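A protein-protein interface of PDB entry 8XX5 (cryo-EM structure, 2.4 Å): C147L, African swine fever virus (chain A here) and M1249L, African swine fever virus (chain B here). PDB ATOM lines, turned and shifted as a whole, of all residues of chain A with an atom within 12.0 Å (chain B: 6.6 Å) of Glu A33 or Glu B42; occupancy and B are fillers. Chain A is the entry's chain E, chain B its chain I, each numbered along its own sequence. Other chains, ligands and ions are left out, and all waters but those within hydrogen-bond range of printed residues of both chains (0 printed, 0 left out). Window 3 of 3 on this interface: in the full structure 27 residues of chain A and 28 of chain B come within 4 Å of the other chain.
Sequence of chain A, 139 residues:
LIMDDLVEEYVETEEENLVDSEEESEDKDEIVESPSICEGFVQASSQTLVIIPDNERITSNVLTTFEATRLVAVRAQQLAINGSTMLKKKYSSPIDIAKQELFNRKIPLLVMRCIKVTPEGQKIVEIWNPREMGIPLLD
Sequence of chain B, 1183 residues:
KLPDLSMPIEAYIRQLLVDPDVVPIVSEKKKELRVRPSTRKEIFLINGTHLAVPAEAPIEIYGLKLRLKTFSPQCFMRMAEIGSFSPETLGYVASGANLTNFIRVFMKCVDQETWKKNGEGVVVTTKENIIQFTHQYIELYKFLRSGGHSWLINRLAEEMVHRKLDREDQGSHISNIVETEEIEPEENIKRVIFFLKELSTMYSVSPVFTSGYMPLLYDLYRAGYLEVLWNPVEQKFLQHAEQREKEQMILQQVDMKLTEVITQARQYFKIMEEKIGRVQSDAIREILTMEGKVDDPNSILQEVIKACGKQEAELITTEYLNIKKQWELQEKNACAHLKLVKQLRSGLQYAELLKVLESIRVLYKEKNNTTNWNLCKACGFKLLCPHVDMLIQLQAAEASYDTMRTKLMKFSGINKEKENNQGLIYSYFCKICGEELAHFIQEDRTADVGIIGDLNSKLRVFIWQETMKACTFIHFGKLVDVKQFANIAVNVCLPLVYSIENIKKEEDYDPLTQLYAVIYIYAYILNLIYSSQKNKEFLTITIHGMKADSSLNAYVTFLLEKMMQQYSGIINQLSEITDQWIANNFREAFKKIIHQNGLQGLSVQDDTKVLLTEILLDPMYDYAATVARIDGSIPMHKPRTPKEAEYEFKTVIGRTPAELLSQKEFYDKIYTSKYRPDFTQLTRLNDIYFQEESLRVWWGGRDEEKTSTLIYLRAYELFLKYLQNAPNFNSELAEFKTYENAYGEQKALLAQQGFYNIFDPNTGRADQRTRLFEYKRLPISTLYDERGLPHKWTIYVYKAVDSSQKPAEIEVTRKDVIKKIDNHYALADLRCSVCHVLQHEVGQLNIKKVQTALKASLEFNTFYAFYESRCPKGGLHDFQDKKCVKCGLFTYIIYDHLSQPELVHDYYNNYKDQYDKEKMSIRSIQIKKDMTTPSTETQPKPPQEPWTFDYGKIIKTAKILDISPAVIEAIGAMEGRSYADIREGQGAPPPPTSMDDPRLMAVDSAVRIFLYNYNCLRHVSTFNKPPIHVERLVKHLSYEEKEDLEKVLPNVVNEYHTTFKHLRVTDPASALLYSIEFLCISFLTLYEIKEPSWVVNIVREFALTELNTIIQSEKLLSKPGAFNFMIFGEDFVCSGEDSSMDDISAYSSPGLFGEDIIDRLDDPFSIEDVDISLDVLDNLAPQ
The guanidinium group (NH2) of Arg B40 lies within salt-bridge range of the side-chain carboxylate (OE1) of Glu A33, 2.7 Å away. The side-chain carboxylate (OE1) of Glu A33 lies close to the side-chain carboxylate (OE1) of Glu B42, 3.1 Å away.
O of Pro B24 is in hydrogen-bond range of N of Phe B44 (3.2 Å). NH2 of Arg B40 lies within salt-bridge range of OE1 of Glu B42. A ring nitrogen (NE2) of His B50 is in hydrogen-bond range of the side-chain carboxylate of Glu B42.
OE2 of Glu A30 touches CZ of Phe B44 (3.98 Å). Glu A33 touches Pro B20 (CG to CB, 3.9 Å). Pro A35 touches Lys B69.
Glu A39 touches none of the printed residues of chain B. No residue of chain A comes within 4 Å of Val B23. Arg B40 touches just one residue of chain A: Glu A33 (2.7 Å). No residue of chain A comes within 4 Å of Lys B41. Of the printed residues of chain A, Glu B42 touches Glu A33 (3.0 Å). No residue of chain A comes within 4 Å of Ile B43. Printed residues of chain A within 4 Å of Phe B44: Glu A30 (3.98 Å). His B50 touches none of the printed residues of chain A. No residue of chain A comes within 4 Å of Ala B52. No residue of chain A comes within 4 Å of Val B53. Of the printed residues of chain A, Lys B69 touches Pro A35 (3.4 Å). The nearest residue of chain A that does not touch Glu B42 is Ile A31 (4.6 Å).
Of the 16 printed residues of chain B, 5 touch a printed residue of chain A. Printed residues of chain B that touch a printed residue of chain A: Pro B20, Arg B40, Glu B42, Phe B44 and Lys B69. Hydrophobic or aromatic side chains of chain B within 4 Å of the printed part of chain A: Pro B20 and Phe B44. Along chain B the printed residues that touch a printed residue of chain A span positions 20 to 69. Among the printed residues, 5 pairs touch across the chains.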
ATOM      1  N   GLU A  30     -30.704  11.923  -9.031  1.00  0.00           N
ATOM      2  CA  GLU A  30     -29.712  12.911  -9.443  1.00  0.00           C
ATOM      3  C   GLU A  30     -29.536  13.981  -8.376  1.00  0.00           C
ATOM      4  O   GLU A  30     -28.424  14.222  -7.906  1.00  0.00           O
ATOM      5  CB  GLU A  30     -30.114  13.554 -10.772  1.00  0.00           C
ATOM      6  CG  GLU A  30     -29.032  14.417 -11.396  1.00  0.00           C
ATOM      7  CD  GLU A  30     -27.649  13.812 -11.253  1.00  0.00           C
ATOM      8  OE1 GLU A  30     -27.317  12.894 -12.032  1.00  0.00           O
ATOM      9  OE2 GLU A  30     -26.890  14.258 -10.366  1.00  0.00           O
ATOM     10  N   ILE A  31     -30.650  14.617  -8.010  1.00  0.00           N
ATOM     11  CA  ILE A  31     -30.704  15.638  -6.969  1.00  0.00           C
ATOM     12  C   ILE A  31     -29.854  16.839  -7.366  1.00  0.00           C
ATOM     13  O   ILE A  31     -28.633  16.847  -7.179  1.00  0.00           O
ATOM     14  CB  ILE A  31     -30.271  15.076  -5.603  1.00  0.00           C
ATOM     15  CG1 ILE A  31     -31.066  13.807  -5.286  1.00  0.00           C
ATOM     16  CG2 ILE A  31     -30.446  16.126  -4.515  1.00  0.00           C
ATOM     17  CD1 ILE A  31     -32.298  14.036  -4.444  1.00  0.00           C
ATOM     18  N   VAL A  32     -30.503  17.862  -7.908  1.00  0.00           N
ATOM     19  CA  VAL A  32     -29.833  19.066  -8.351  1.00  0.00           C
ATOM     20  C   VAL A  32     -30.112  20.163  -7.328  1.00  0.00           C
ATOM     21  O   VAL A  32     -30.838  19.965  -6.357  1.00  0.00           O
ATOM     22  CB  VAL A  32     -30.276  19.472  -9.780  1.00  0.00           C
ATOM     23  CG1 VAL A  32     -29.234  20.362 -10.452  1.00  0.00           C
ATOM     24  CG2 VAL A  32     -30.543  18.234 -10.620  1.00  0.00           C
ATOM     25  N   GLU A  33     -29.506  21.335  -7.533  1.00  0.00           N
ATOM     26  CA  GLU A  33     -29.574  22.427  -6.567  1.00  0.00           C
ATOM     27  C   GLU A  33     -31.012  22.779  -6.216  1.00  0.00           C
ATOM     28  O   GLU A  33     -31.448  22.565  -5.080  1.00  0.00           O
ATOM     29  CB  GLU A  33     -28.871  23.668  -7.125  1.00  0.00           C
ATOM     30  CG  GLU A  33     -27.696  23.371  -8.046  1.00  0.00           C
ATOM     31  CD  GLU A  33     -26.384  23.226  -7.301  1.00  0.00           C
ATOM     32  OE1 GLU A  33     -26.404  22.764  -6.142  1.00  0.00           O
ATOM     33  OE2 GLU A  33     -25.332  23.577  -7.875  1.00  0.00           O
ATOM     34  N   SER A  34     -31.757  23.300  -7.186  1.00  0.00           N
ATOM     35  CA  SER A  34     -33.182  23.565  -7.045  1.00  0.00           C
ATOM     36  C   SER A  34     -33.748  23.989  -8.392  1.00  0.00           C
ATOM     37  O   SER A  34     -33.135  24.805  -9.093  1.00  0.00           O
ATOM     38  CB  SER A  34     -33.444  24.649  -5.997  1.00  0.00           C
ATOM     39  OG  SER A  34     -33.382  24.112  -4.686  1.00  0.00           O
ATOM     40  N   PRO A  35     -34.898  23.465  -8.793  1.00  0.00           N
ATOM     41  CA  PRO A  35     -35.550  23.978 -10.001  1.00  0.00           C
ATOM     42  C   PRO A  35     -36.471  25.138  -9.672  1.00  0.00           C
ATOM     43  O   PRO A  35     -36.612  25.513  -8.504  1.00  0.00           O
ATOM     44  CB  PRO A  35     -36.328  22.764 -10.532  1.00  0.00           C
ATOM     45  CG  PRO A  35     -36.145  21.655  -9.496  1.00  0.00           C
ATOM     46  CD  PRO A  35     -35.590  22.285  -8.260  1.00  0.00           C
ATOM     47  N   SER A  36     -37.102  25.717 -10.688  1.00  0.00           N
ATOM     48  CA  SER A  36     -38.090  26.761 -10.468  1.00  0.00           C
ATOM     49  C   SER A  36     -39.455  26.205 -10.089  1.00  0.00           C
ATOM     50  O   SER A  36     -40.442  26.947 -10.126  1.00  0.00           O
ATOM     51  CB  SER A  36     -38.214  27.640 -11.715  1.00  0.00           C
ATOM     52  OG  SER A  36     -38.534  28.976 -11.367  1.00  0.00           O
ATOM     53  N   ILE A  37     -39.536  24.925  -9.726  1.00  0.00           N
ATOM     54  CA  ILE A  37     -40.802  24.266  -9.421  1.00  0.00           C
ATOM     55  C   ILE A  37     -40.816  23.715  -7.993  1.00  0.00           C
ATOM     56  O   ILE A  37     -41.728  24.007  -7.218  1.00  0.00           O
ATOM     57  CB  ILE A  37     -41.118  23.163 -10.457  1.00  0.00           C
ATOM     58  CG1 ILE A  37     -39.992  22.133 -10.545  1.00  0.00           C
ATOM     59  CG2 ILE A  37     -41.289  23.787 -11.823  1.00  0.00           C
ATOM     60  CD1 ILE A  37     -40.128  21.180 -11.707  1.00  0.00           C
ATOM     61  N   CYS A  38     -39.813  22.911  -7.632  1.00  0.00           N
ATOM     62  CA  CYS A  38     -39.761  22.352  -6.284  1.00  0.00           C
ATOM     63  C   CYS A  38     -39.527  23.447  -5.253  1.00  0.00           C
ATOM     64  O   CYS A  38     -40.251  23.539  -4.255  1.00  0.00           O
ATOM     65  CB  CYS A  38     -38.669  21.284  -6.202  1.00  0.00           C
ATOM     66  SG  CYS A  38     -39.010  19.959  -5.017  1.00  0.00           S
ATOM     67  N   GLU A  39     -38.522  24.287  -5.480  1.00  0.00           N
ATOM     68  CA  GLU A  39     -38.292  25.471  -4.660  1.00  0.00           C
ATOM     69  C   GLU A  39     -39.081  26.620  -5.275  1.00  0.00           C
ATOM     70  O   GLU A  39     -38.831  27.013  -6.420  1.00  0.00           O
ATOM     71  CB  GLU A  39     -36.804  25.799  -4.575  1.00  0.00           C
ATOM     72  CG  GLU A  39     -36.494  27.236  -4.163  1.00  0.00           C
ATOM     73  CD  GLU A  39     -37.006  27.584  -2.775  1.00  0.00           C
ATOM     74  OE1 GLU A  39     -38.198  27.931  -2.642  1.00  0.00           O
ATOM     75  OE2 GLU A  39     -36.212  27.510  -1.814  1.00  0.00           O
ATOM     76  N   GLY A  40     -40.030  27.150  -4.524  1.00  0.00           N
ATOM     77  CA  GLY A  40     -40.923  28.183  -5.001  1.00  0.00           C
ATOM     78  C   GLY A  40     -42.329  27.649  -5.170  1.00  0.00           C
ATOM     79  O   GLY A  40     -42.724  26.649  -4.564  1.00  0.00           O
ATOM     80  N   LEU B  17     -20.867  28.808 -15.506  1.00  0.00           N
ATOM     81  CA  LEU B  17     -21.092  28.030 -14.294  1.00  0.00           C
ATOM     82  C   LEU B  17     -22.062  28.708 -13.336  1.00  0.00           C
ATOM     83  O   LEU B  17     -22.524  28.064 -12.390  1.00  0.00           O
ATOM     84  CB  LEU B  17     -19.763  27.766 -13.586  1.00  0.00           C
ATOM     85  CG  LEU B  17     -18.677  27.085 -14.417  1.00  0.00           C
ATOM     86  CD1 LEU B  17     -17.347  27.108 -13.684  1.00  0.00           C
ATOM     87  CD2 LEU B  17     -19.078  25.663 -14.772  1.00  0.00           C
ATOM     88  N   PRO B  20     -27.041  26.848 -12.816  1.00  0.00           N
ATOM     89  CA  PRO B  20     -26.958  25.510 -12.206  1.00  0.00           C
ATOM     90  C   PRO B  20     -26.966  24.365 -13.205  1.00  0.00           C
ATOM     91  O   PRO B  20     -26.418  23.300 -12.896  1.00  0.00           O
ATOM     92  CB  PRO B  20     -28.190  25.464 -11.290  1.00  0.00           C
ATOM     93  CG  PRO B  20     -29.093  26.553 -11.791  1.00  0.00           C
ATOM     94  CD  PRO B  20     -28.179  27.621 -12.292  1.00  0.00           C
ATOM     95  N   ASP B  21     -27.567  24.534 -14.386  1.00  0.00           N
ATOM     96  CA  ASP B  21     -27.606  23.431 -15.342  1.00  0.00           C
ATOM     97  C   ASP B  21     -26.230  23.135 -15.924  1.00  0.00           C
ATOM     98  O   ASP B  21     -25.931  21.980 -16.243  1.00  0.00           O
ATOM     99  CB  ASP B  21     -28.599  23.724 -16.469  1.00  0.00           C
ATOM    100  CG  ASP B  21     -29.799  24.515 -15.999  1.00  0.00           C
ATOM    101  OD1 ASP B  21     -30.484  24.059 -15.062  1.00  0.00           O
ATOM    102  OD2 ASP B  21     -30.053  25.601 -16.557  1.00  0.00           O
ATOM    103  N   VAL B  22     -25.389  24.152 -16.077  1.00  0.00           N
ATOM    104  CA  VAL B  22     -24.040  23.963 -16.598  1.00  0.00           C
ATOM    105  C   VAL B  22     -23.160  23.475 -15.453  1.00  0.00           C
ATOM    106  O   VAL B  22     -22.828  24.239 -14.543  1.00  0.00           O
ATOM    107  CB  VAL B  22     -23.485  25.253 -17.212  1.00  0.00           C
ATOM    108  CG1 VAL B  22     -21.993  25.120 -17.479  1.00  0.00           C
ATOM    109  CG2 VAL B  22     -24.230  25.595 -18.489  1.00  0.00           C
ATOM    110  N   VAL B  23     -22.787  22.199 -15.488  1.00  0.00           N
ATOM    111  CA  VAL B  23     -21.895  21.641 -14.476  1.00  0.00           C
ATOM    112  C   VAL B  23     -20.558  21.317 -15.133  1.00  0.00           C
ATOM    113  O   VAL B  23     -20.521  20.914 -16.305  1.00  0.00           O
ATOM    114  CB  VAL B  23     -22.514  20.407 -13.796  1.00  0.00           C
ATOM    115  CG1 VAL B  23     -23.918  20.723 -13.309  1.00  0.00           C
ATOM    116  CG2 VAL B  23     -22.535  19.214 -14.738  1.00  0.00           C
ATOM    117  N   PRO B  24     -19.443  21.513 -14.442  1.00  0.00           N
ATOM    118  CA  PRO B  24     -18.135  21.205 -15.021  1.00  0.00           C
ATOM    119  C   PRO B  24     -17.661  19.797 -14.675  1.00  0.00           C
ATOM    120  O   PRO B  24     -18.225  19.107 -13.824  1.00  0.00           O
ATOM    121  CB  PRO B  24     -17.226  22.258 -14.381  1.00  0.00           C
ATOM    122  CG  PRO B  24     -17.841  22.512 -13.051  1.00  0.00           C
ATOM    123  CD  PRO B  24     -19.325  22.260 -13.178  1.00  0.00           C
ATOM    124  N   ARG B  40     -20.753  29.447  -5.162  1.00  0.00           N
ATOM    125  CA  ARG B  40     -20.615  28.031  -4.850  1.00  0.00           C
ATOM    126  C   ARG B  40     -21.162  27.190  -5.995  1.00  0.00           C
ATOM    127  O   ARG B  40     -22.268  27.432  -6.486  1.00  0.00           O
ATOM    128  CB  ARG B  40     -21.350  27.713  -3.550  1.00  0.00           C
ATOM    129  CG  ARG B  40     -21.349  26.250  -3.168  1.00  0.00           C
ATOM    130  CD  ARG B  40     -22.615  25.880  -2.413  1.00  0.00           C
ATOM    131  NE  ARG B  40     -23.600  25.241  -3.275  1.00  0.00           N
ATOM    132  CZ  ARG B  40     -23.864  23.941  -3.272  1.00  0.00           C
ATOM    133  NH1 ARG B  40     -23.238  23.112  -2.454  1.00  0.00           N
ATOM    134  NH2 ARG B  40     -24.781  23.463  -4.106  1.00  0.00           N
ATOM    135  N   LYS B  41     -20.384  26.200  -6.423  1.00  0.00           N
ATOM    136  CA  LYS B  41     -20.730  25.398  -7.587  1.00  0.00           C
ATOM    137  C   LYS B  41     -20.544  23.921  -7.285  1.00  0.00           C
ATOM    138  O   LYS B  41     -19.552  23.523  -6.667  1.00  0.00           O
ATOM    139  CB  LYS B  41     -19.876  25.791  -8.800  1.00  0.00           C
ATOM    140  CG  LYS B  41     -20.399  25.254 -10.118  1.00  0.00           C
ATOM    141  CD  LYS B  41     -21.829  25.702 -10.345  1.00  0.00           C
ATOM    142  CE  LYS B  41     -22.478  24.937 -11.479  1.00  0.00           C
ATOM    143  NZ  LYS B  41     -21.546  24.747 -12.620  1.00  0.00           N
ATOM    144  N   GLU B  42     -21.502  23.112  -7.725  1.00  0.00           N
ATOM    145  CA  GLU B  42     -21.373  21.665  -7.666  1.00  0.00           C
ATOM    146  C   GLU B  42     -20.694  21.162  -8.932  1.00  0.00           C
ATOM    147  O   GLU B  42     -21.032  21.580 -10.042  1.00  0.00           O
ATOM    148  CB  GLU B  42     -22.737  20.994  -7.499  1.00  0.00           C
ATOM    149  CG  GLU B  42     -23.428  21.316  -6.187  1.00  0.00           C
ATOM    150  CD  GLU B  42     -24.582  20.378  -5.888  1.00  0.00           C
ATOM    151  OE1 GLU B  42     -25.067  20.379  -4.738  1.00  0.00           O
ATOM    152  OE2 GLU B  42     -25.005  19.642  -6.804  1.00  0.00           O
ATOM    153  N   ILE B  43     -19.727  20.265  -8.754  1.00  0.00           N
ATOM    154  CA  ILE B  43     -18.892  19.776  -9.839  1.00  0.00           C
ATOM    155  C   ILE B  43     -18.934  18.254  -9.849  1.00  0.00           C
ATOM    156  O   ILE B  43     -19.437  17.613  -8.927  1.00  0.00           O
ATOM    157  CB  ILE B  43     -17.433  20.263  -9.720  1.00  0.00           C
ATOM    158  CG1 ILE B  43     -16.725  19.513  -8.590  1.00  0.00           C
ATOM    159  CG2 ILE B  43     -17.382  21.762  -9.481  1.00  0.00           C
ATOM    160  CD1 ILE B  43     -15.326  19.999  -8.306  1.00  0.00           C
ATOM    161  N   PHE B  44     -18.398  17.684 -10.922  1.00  0.00           N
ATOM    162  CA  PHE B  44     -18.134  16.257 -11.017  1.00  0.00           C
ATOM    163  C   PHE B  44     -16.665  16.054 -11.353  1.00  0.00           C
ATOM    164  O   PHE B  44     -16.112  16.762 -12.200  1.00  0.00           O
ATOM    165  CB  PHE B  44     -18.998  15.589 -12.085  1.00  0.00           C
ATOM    166  CG  PHE B  44     -20.458  15.537 -11.748  1.00  0.00           C
ATOM    167  CD1 PHE B  44     -20.983  14.459 -11.058  1.00  0.00           C
ATOM    168  CD2 PHE B  44     -21.308  16.559 -12.127  1.00  0.00           C
ATOM    169  CE1 PHE B  44     -22.326  14.406 -10.748  1.00  0.00           C
ATOM    170  CE2 PHE B  44     -22.652  16.511 -11.821  1.00  0.00           C
ATOM    171  CZ  PHE B  44     -23.162  15.433 -11.130  1.00  0.00           C
ATOM    172  N   HIS B  50     -19.386  13.271  -7.236  1.00  0.00           N
ATOM    173  CA  HIS B  50     -20.057  14.563  -7.234  1.00  0.00           C
ATOM    174  C   HIS B  50     -19.639  15.340  -5.992  1.00  0.00           C
ATOM    175  O   HIS B  50     -19.810  14.857  -4.868  1.00  0.00           O
ATOM    176  CB  HIS B  50     -21.573  14.374  -7.272  1.00  0.00           C
ATOM    177  CG  HIS B  50     -22.342  15.652  -7.389  1.00  0.00           C
ATOM    178  ND1 HIS B  50     -22.035  16.623  -8.317  1.00  0.00           N
ATOM    179  CD2 HIS B  50     -23.413  16.113  -6.702  1.00  0.00           C
ATOM    180  CE1 HIS B  50     -22.881  17.630  -8.193  1.00  0.00           C
ATOM    181  NE2 HIS B  50     -23.727  17.347  -7.220  1.00  0.00           N
ATOM    182  N   LEU B  51     -19.094  16.536  -6.196  1.00  0.00           N
ATOM    183  CA  LEU B  51     -18.660  17.396  -5.105  1.00  0.00           C
ATOM    184  C   LEU B  51     -19.106  18.826  -5.371  1.00  0.00           C
ATOM    185  O   LEU B  51     -19.650  19.149  -6.429  1.00  0.00           O
ATOM    186  CB  LEU B  51     -17.138  17.350  -4.915  1.00  0.00           C
ATOM    187  CG  LEU B  51     -16.495  15.999  -4.599  1.00  0.00           C
ATOM    188  CD1 LEU B  51     -15.883  15.394  -5.848  1.00  0.00           C
ATOM    189  CD2 LEU B  51     -15.453  16.155  -3.508  1.00  0.00           C
ATOM    190  N   ALA B  52     -18.868  19.684  -4.386  1.00  0.00           N
ATOM    191  CA  ALA B  52     -19.148  21.107  -4.489  1.00  0.00           C
ATOM    192  C   ALA B  52     -17.927  21.886  -4.033  1.00  0.00           C
ATOM    193  O   ALA B  52     -17.269  21.508  -3.060  1.00  0.00           O
ATOM    194  CB  ALA B  52     -20.369  21.504  -3.654  1.00  0.00           C
ATOM    195  N   VAL B  53     -17.623  22.969  -4.740  1.00  0.00           N
ATOM    196  CA  VAL B  53     -16.474  23.806  -4.405  1.00  0.00           C
ATOM    197  C   VAL B  53     -16.974  25.165  -3.933  1.00  0.00           C
ATOM    198  O   VAL B  53     -18.048  25.611  -4.361  1.00  0.00           O
ATOM    199  CB  VAL B  53     -15.522  23.947  -5.603  1.00  0.00           C
ATOM    200  CG1 VAL B  53     -14.821  22.627  -5.876  1.00  0.00           C
ATOM    201  CG2 VAL B  53     -16.279  24.419  -6.832  1.00  0.00           C
ATOM    202  N   LYS B  69     -32.720  19.501 -17.884  1.00  0.00           N
ATOM    203  CA  LYS B  69     -33.743  19.278 -16.872  1.00  0.00           C
ATOM    204  C   LYS B  69     -35.096  19.026 -17.524  1.00  0.00           C
ATOM    205  O   LYS B  69     -35.447  19.647 -18.530  1.00  0.00           O
ATOM    206  CB  LYS B  69     -33.828  20.478 -15.929  1.00  0.00           C
ATOM    207  CG  LYS B  69     -32.481  21.034 -15.506  1.00  0.00           C
ATOM    208  CD  LYS B  69     -32.603  21.857 -14.235  1.00  0.00           C
ATOM    209  CE  LYS B  69     -33.028  21.002 -13.056  1.00  0.00           C
ATOM    210  NZ  LYS B  69     -33.371  21.834 -11.870  1.00  0.00           N
